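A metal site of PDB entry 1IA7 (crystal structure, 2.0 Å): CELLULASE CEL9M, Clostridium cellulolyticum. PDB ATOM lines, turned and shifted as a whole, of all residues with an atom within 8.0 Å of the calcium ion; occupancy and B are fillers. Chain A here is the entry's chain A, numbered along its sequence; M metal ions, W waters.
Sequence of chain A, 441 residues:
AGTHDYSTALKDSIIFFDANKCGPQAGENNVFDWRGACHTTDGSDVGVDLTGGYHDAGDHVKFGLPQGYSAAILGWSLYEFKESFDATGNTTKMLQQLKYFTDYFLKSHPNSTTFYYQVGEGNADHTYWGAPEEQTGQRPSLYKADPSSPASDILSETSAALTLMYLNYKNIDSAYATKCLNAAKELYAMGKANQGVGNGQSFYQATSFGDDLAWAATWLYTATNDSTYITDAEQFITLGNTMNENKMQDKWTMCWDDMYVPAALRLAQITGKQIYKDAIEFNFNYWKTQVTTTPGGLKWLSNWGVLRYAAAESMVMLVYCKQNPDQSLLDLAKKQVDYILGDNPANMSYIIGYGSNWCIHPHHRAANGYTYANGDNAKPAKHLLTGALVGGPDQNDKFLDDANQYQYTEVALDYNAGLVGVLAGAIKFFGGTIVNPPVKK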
ATOM      1  N   LEU A  65     -13.910  17.602  -2.274  1.00  0.00           N
ATOM      2  CA  LEU A  65     -14.010  17.733  -0.822  1.00  0.00           C
ATOM      3  C   LEU A  65     -13.064  18.793  -0.253  1.00  0.00           C
ATOM      4  O   LEU A  65     -13.496  19.697   0.461  1.00  0.00           O
ATOM      5  CB  LEU A  65     -13.792  16.375  -0.139  1.00  0.00           C
ATOM      6  CG  LEU A  65     -13.977  16.310   1.386  1.00  0.00           C
ATOM      7  CD1 LEU A  65     -15.251  17.046   1.818  1.00  0.00           C
ATOM      8  CD2 LEU A  65     -14.029  14.843   1.833  1.00  0.00           C
ATOM      9  N   SER A 152     -22.751  13.746  -0.295  1.00  0.00           N
ATOM     10  CA  SER A 152     -23.247  14.596   0.785  1.00  0.00           C
ATOM     11  C   SER A 152     -22.208  15.464   1.470  1.00  0.00           C
ATOM     12  O   SER A 152     -22.485  16.624   1.787  1.00  0.00           O
ATOM     13  CB  SER A 152     -23.962  13.728   1.834  1.00  0.00           C
ATOM     14  OG  SER A 152     -24.927  12.904   1.209  1.00  0.00           O
ATOM     15  N   ASP A 153     -21.024  14.925   1.707  1.00  0.00           N
ATOM     16  CA  ASP A 153     -19.984  15.720   2.368  1.00  0.00           C
ATOM     17  C   ASP A 153     -19.476  16.835   1.458  1.00  0.00           C
ATOM     18  O   ASP A 153     -19.400  17.992   1.867  1.00  0.00           O
ATOM     19  CB  ASP A 153     -18.840  14.814   2.860  1.00  0.00           C
ATOM     20  CG  ASP A 153     -18.294  13.900   1.767  1.00  0.00           C
ATOM     21  OD1 ASP A 153     -18.975  13.692   0.745  1.00  0.00           O
ATOM     22  OD2 ASP A 153     -17.182  13.359   1.963  1.00  0.00           O
ATOM     23  N   ILE A 154     -19.144  16.499   0.222  1.00  0.00           N
ATOM     24  CA  ILE A 154     -18.660  17.501  -0.731  1.00  0.00           C
ATOM     25  C   ILE A 154     -19.732  18.568  -0.967  1.00  0.00           C
ATOM     26  O   ILE A 154     -19.458  19.769  -0.904  1.00  0.00           O
ATOM     27  CB  ILE A 154     -18.272  16.831  -2.072  1.00  0.00           C
ATOM     28  CG1 ILE A 154     -17.143  15.832  -1.823  1.00  0.00           C
ATOM     29  CG2 ILE A 154     -17.839  17.888  -3.086  1.00  0.00           C
ATOM     30  CD1 ILE A 154     -16.679  15.087  -3.056  1.00  0.00           C
ATOM     31  N   GLU A 157     -20.038  20.926   2.192  1.00  0.00           N
ATOM     32  CA  GLU A 157     -18.955  21.893   2.408  1.00  0.00           C
ATOM     33  C   GLU A 157     -19.048  23.008   1.372  1.00  0.00           C
ATOM     34  O   GLU A 157     -18.827  24.181   1.683  1.00  0.00           O
ATOM     35  CB  GLU A 157     -17.592  21.203   2.342  1.00  0.00           C
ATOM     36  CG  GLU A 157     -17.261  20.377   3.588  1.00  0.00           C
ATOM     37  CD  GLU A 157     -17.459  21.152   4.880  1.00  0.00           C
ATOM     38  OE1 GLU A 157     -17.105  22.349   4.922  1.00  0.00           O
ATOM     39  OE2 GLU A 157     -17.967  20.579   5.865  1.00  0.00           O
ATOM     40  N   VAL A 197     -20.890   9.520   1.080  1.00  0.00           N
ATOM     41  CA  VAL A 197     -19.717  10.350   0.831  1.00  0.00           C
ATOM     42  C   VAL A 197     -19.404  10.364  -0.652  1.00  0.00           C
ATOM     43  O   VAL A 197     -19.678   9.401  -1.371  1.00  0.00           O
ATOM     44  CB  VAL A 197     -18.468   9.828   1.593  1.00  0.00           C
ATOM     45  CG1 VAL A 197     -18.700   9.902   3.093  1.00  0.00           C
ATOM     46  CG2 VAL A 197     -18.155   8.406   1.154  1.00  0.00           C
ATOM     47  N   ALA A 206     -13.072   9.724   1.868  1.00  0.00           N
ATOM     48  CA  ALA A 206     -13.938  10.247   2.912  1.00  0.00           C
ATOM     49  C   ALA A 206     -14.531   9.137   3.772  1.00  0.00           C
ATOM     50  O   ALA A 206     -14.691   8.005   3.326  1.00  0.00           O
ATOM     51  CB  ALA A 206     -15.055  11.067   2.292  1.00  0.00           C
ATOM     52  N   THR A 207     -14.845   9.479   5.019  1.00  0.00           N
ATOM     53  CA  THR A 207     -15.412   8.522   5.950  1.00  0.00           C
ATOM     54  C   THR A 207     -16.665   9.025   6.663  1.00  0.00           C
ATOM     55  O   THR A 207     -17.298   8.287   7.401  1.00  0.00           O
ATOM     56  CB  THR A 207     -14.378   8.153   7.035  1.00  0.00           C
ATOM     57  OG1 THR A 207     -14.117   9.305   7.842  1.00  0.00           O
ATOM     58  CG2 THR A 207     -13.074   7.692   6.402  1.00  0.00           C
ATOM     59  N   SER A 208     -17.029  10.295   6.440  1.00  0.00           N
ATOM     60  CA  SER A 208     -18.208  10.837   7.120  1.00  0.00           C
ATOM     61  C   SER A 208     -18.894  11.974   6.380  1.00  0.00           C
ATOM     62  O   SER A 208     -18.245  12.767   5.683  1.00  0.00           O
ATOM     63  CB  SER A 208     -17.784  11.339   8.504  1.00  0.00           C
ATOM     64  OG  SER A 208     -16.889  12.435   8.367  1.00  0.00           O
ATOM     65  N   PHE A 209     -20.209  12.080   6.526  1.00  0.00           N
ATOM     66  CA  PHE A 209     -20.947  13.163   5.888  1.00  0.00           C
ATOM     67  C   PHE A 209     -21.963  13.829   6.827  1.00  0.00           C
ATOM     68  O   PHE A 209     -22.392  14.949   6.595  1.00  0.00           O
ATOM     69  CB  PHE A 209     -21.638  12.681   4.587  1.00  0.00           C
ATOM     70  CG  PHE A 209     -22.684  11.617   4.791  1.00  0.00           C
ATOM     71  CD1 PHE A 209     -23.942  11.951   5.267  1.00  0.00           C
ATOM     72  CD2 PHE A 209     -22.401  10.288   4.493  1.00  0.00           C
ATOM     73  CE1 PHE A 209     -24.925  10.977   5.438  1.00  0.00           C
ATOM     74  CE2 PHE A 209     -23.380   9.304   4.662  1.00  0.00           C
ATOM     75  CZ  PHE A 209     -24.642   9.648   5.140  1.00  0.00           C
ATOM     76  N   GLY A 210     -22.333  13.122   7.899  1.00  0.00           N
ATOM     77  CA  GLY A 210     -23.268  13.698   8.852  1.00  0.00           C
ATOM     78  C   GLY A 210     -22.715  14.981   9.432  1.00  0.00           C
ATOM     79  O   GLY A 210     -23.455  15.932   9.705  1.00  0.00           O
ATOM     80  N   ASP A 211     -21.401  15.009   9.628  1.00  0.00           N
ATOM     81  CA  ASP A 211     -20.736  16.193  10.169  1.00  0.00           C
ATOM     82  C   ASP A 211     -20.906  17.369   9.216  1.00  0.00           C
ATOM     83  O   ASP A 211     -21.198  18.492   9.637  1.00  0.00           O
ATOM     84  CB  ASP A 211     -19.246  15.885  10.382  1.00  0.00           C
ATOM     85  CG  ASP A 211     -18.571  15.314   9.144  1.00  0.00           C
ATOM     86  OD1 ASP A 211     -19.180  14.456   8.484  1.00  0.00           O
ATOM     87  OD2 ASP A 211     -17.425  15.706   8.850  1.00  0.00           O
ATOM     88  N   ASP A 212     -20.740  17.103   7.922  1.00  0.00           N
ATOM     89  CA  ASP A 212     -20.842  18.132   6.910  1.00  0.00           C
ATOM     90  C   ASP A 212     -22.271  18.673   6.722  1.00  0.00           C
ATOM     91  O   ASP A 212     -22.467  19.890   6.592  1.00  0.00           O
ATOM     92  CB  ASP A 212     -20.282  17.590   5.595  1.00  0.00           C
ATOM     93  CG  ASP A 212     -18.835  17.141   5.749  1.00  0.00           C
ATOM     94  OD1 ASP A 212     -17.946  18.014   5.884  1.00  0.00           O
ATOM     95  OD2 ASP A 212     -18.591  15.914   5.756  1.00  0.00           O
ATOM     96  N   LEU A 213     -23.260  17.775   6.714  1.00  0.00           N
ATOM     97  CA  LEU A 213     -24.656  18.180   6.561  1.00  0.00           C
ATOM     98  C   LEU A 213     -25.044  19.120   7.711  1.00  0.00           C
ATOM     99  O   LEU A 213     -25.669  20.163   7.483  1.00  0.00           O
ATOM    100  CB  LEU A 213     -25.580  16.952   6.571  1.00  0.00           C
ATOM    101  CG  LEU A 213     -25.584  16.055   5.326  1.00  0.00           C
ATOM    102  CD1 LEU A 213     -26.388  14.795   5.605  1.00  0.00           C
ATOM    103  CD2 LEU A 213     -26.174  16.808   4.145  1.00  0.00           C
ATOM    104  N   CYS A 255     -10.894  19.327   9.757  1.00  0.00           N
ATOM    105  CA  CYS A 255     -10.139  19.019   8.550  1.00  0.00           C
ATOM    106  C   CYS A 255     -11.120  18.661   7.435  1.00  0.00           C
ATOM    107  O   CYS A 255     -12.308  18.501   7.692  1.00  0.00           O
ATOM    108  CB  CYS A 255      -9.137  17.886   8.792  1.00  0.00           C
ATOM    109  SG  CYS A 255      -9.861  16.265   9.053  1.00  0.00           S
ATOM    110  N   TRP A 256     -10.629  18.538   6.211  1.00  0.00           N
ATOM    111  CA  TRP A 256     -11.494  18.246   5.080  1.00  0.00           C
ATOM    112  C   TRP A 256     -12.448  17.054   5.239  1.00  0.00           C
ATOM    113  O   TRP A 256     -13.537  17.064   4.674  1.00  0.00           O
ATOM    114  CB  TRP A 256     -10.675  18.062   3.785  1.00  0.00           C
ATOM    115  CG  TRP A 256      -9.623  16.980   3.824  1.00  0.00           C
ATOM    116  CD1 TRP A 256      -8.301  17.142   4.148  1.00  0.00           C
ATOM    117  CD2 TRP A 256      -9.795  15.592   3.521  1.00  0.00           C
ATOM    118  NE1 TRP A 256      -7.644  15.938   4.070  1.00  0.00           N
ATOM    119  CE2 TRP A 256      -8.535  14.967   3.692  1.00  0.00           C
ATOM    120  CE3 TRP A 256     -10.887  14.811   3.128  1.00  0.00           C
ATOM    121  CZ2 TRP A 256      -8.349  13.588   3.484  1.00  0.00           C
ATOM    122  CZ3 TRP A 256     -10.704  13.443   2.913  1.00  0.00           C
ATOM    123  CH2 TRP A 256      -9.439  12.851   3.100  1.00  0.00           C
ATOM    124  N   ASP A 257     -12.042  16.052   6.013  1.00  0.00           N
ATOM    125  CA  ASP A 257     -12.883  14.868   6.215  1.00  0.00           C
ATOM    126  C   ASP A 257     -13.679  14.872   7.516  1.00  0.00           C
ATOM    127  O   ASP A 257     -14.675  14.170   7.628  1.00  0.00           O
ATOM    128  CB  ASP A 257     -12.005  13.604   6.157  1.00  0.00           C
ATOM    129  CG  ASP A 257     -12.807  12.305   6.235  1.00  0.00           C
ATOM    130  OD1 ASP A 257     -13.784  12.169   5.479  1.00  0.00           O
ATOM    131  OD2 ASP A 257     -12.444  11.422   7.043  1.00  0.00           O
ATOM    132  N   ASP A 258     -13.263  15.683   8.492  1.00  0.00           N
ATOM    133  CA  ASP A 258     -13.942  15.718   9.789  1.00  0.00           C
ATOM    134  C   ASP A 258     -14.351  17.102  10.261  1.00  0.00           C
ATOM    135  O   ASP A 258     -13.526  17.912  10.688  1.00  0.00           O
ATOM    136  CB  ASP A 258     -13.044  15.042  10.823  1.00  0.00           C
ATOM    137  CG  ASP A 258     -13.617  15.115  12.230  1.00  0.00           C
ATOM    138  OD1 ASP A 258     -14.833  15.321  12.376  1.00  0.00           O
ATOM    139  OD2 ASP A 258     -12.833  14.949  13.181  1.00  0.00           O
ATOM    140  N   MET A 259     -15.654  17.374  10.204  1.00  0.00           N
ATOM    141  CA  MET A 259     -16.175  18.672  10.628  1.00  0.00           C
ATOM    142  C   MET A 259     -17.110  18.589  11.829  1.00  0.00           C
ATOM    143  O   MET A 259     -17.944  19.464  12.047  1.00  0.00           O
ATOM    144  CB  MET A 259     -16.894  19.345   9.451  1.00  0.00           C
ATOM    145  CG  MET A 259     -15.946  19.876   8.379  1.00  0.00           C
ATOM    146  SD  MET A 259     -14.948  21.263   8.991  1.00  0.00           S
ATOM    147  CE  MET A 259     -16.159  22.598   8.888  1.00  0.00           C
ATOM    148  N   TYR A 260     -16.948  17.539  12.634  1.00  0.00           N
ATOM    149  CA  TYR A 260     -17.789  17.367  13.818  1.00  0.00           C
ATOM    150  C   TYR A 260     -17.576  18.422  14.902  1.00  0.00           C
ATOM    151  O   TYR A 260     -18.523  18.774  15.607  1.00  0.00           O
ATOM    152  CB  TYR A 260     -17.569  15.971  14.413  1.00  0.00           C
ATOM    153  CG  TYR A 260     -18.253  14.880  13.636  1.00  0.00           C
ATOM    154  CD1 TYR A 260     -19.646  14.765  13.646  1.00  0.00           C
ATOM    155  CD2 TYR A 260     -17.521  13.977  12.862  1.00  0.00           C
ATOM    156  CE1 TYR A 260     -20.289  13.776  12.899  1.00  0.00           C
ATOM    157  CE2 TYR A 260     -18.154  12.992  12.116  1.00  0.00           C
ATOM    158  CZ  TYR A 260     -19.538  12.903  12.132  1.00  0.00           C
ATOM    159  OH  TYR A 260     -20.174  11.952  11.372  1.00  0.00           O
HETATM  160 CA    CA M   1     -16.840  14.467   6.828  1.00  0.00          CA
HETATM  161  O   HOH W   1     -15.742  16.448   6.263  1.00  0.00           O
HETATM  162  O   HOH W   2     -15.847  13.796   4.828  1.00  0.00           O
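The calcium ion is bound by the backbone carbonyl oxygen (O) of Asp 257 (2.3 Å), water W2 (2.3 Å), water W1 (2.3 Å), the side-chain carboxylate (OD2) of Asp 211 (2.4 Å), the backbone carbonyl oxygen (O) of Ser 208 (2.5 Å), the side-chain carboxylate (OD2) of Asp 212 (2.5 Å), the side-chain hydroxyl (OG) of Ser 208 (2.5 Å) and the side-chain carboxylate (OD1) of Asp 211 (2.9 Å). The calcium ion has eight donor atoms within binding distance.
OD2 of Asp 257 lies within hydrogen-bond range of OG1 of Thr 207 (2.8 Å). SG of Cys 255 lies close to N of Asp 257 (3.7 Å). The backbone NH (N) of Phe 209 lies close to the side-chain carboxylate (OD1) of Asp 211 (3.2 Å). The side-chain carboxylate (OD2) of Asp 211 lies close to the backbone NH (N) of Met 259 (2.8 Å). OD1 of Asp 212 lies close to OE2 of Glu 157 (2.6 Å).
Within 4 Å of the calcium ion: Ser 208, Asp 211, Asp 212 and Asp 257.
Water W2 bridges the side-chain carboxylate (OD1) of Asp 257 (2.7 Å) and the side-chain carboxylate (OD2) of Asp 153 (3.2 Å). Water W1 lies within hydrogen-bond range of OD1 of Asp 212, O of Trp 256 and N of Asp 258.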
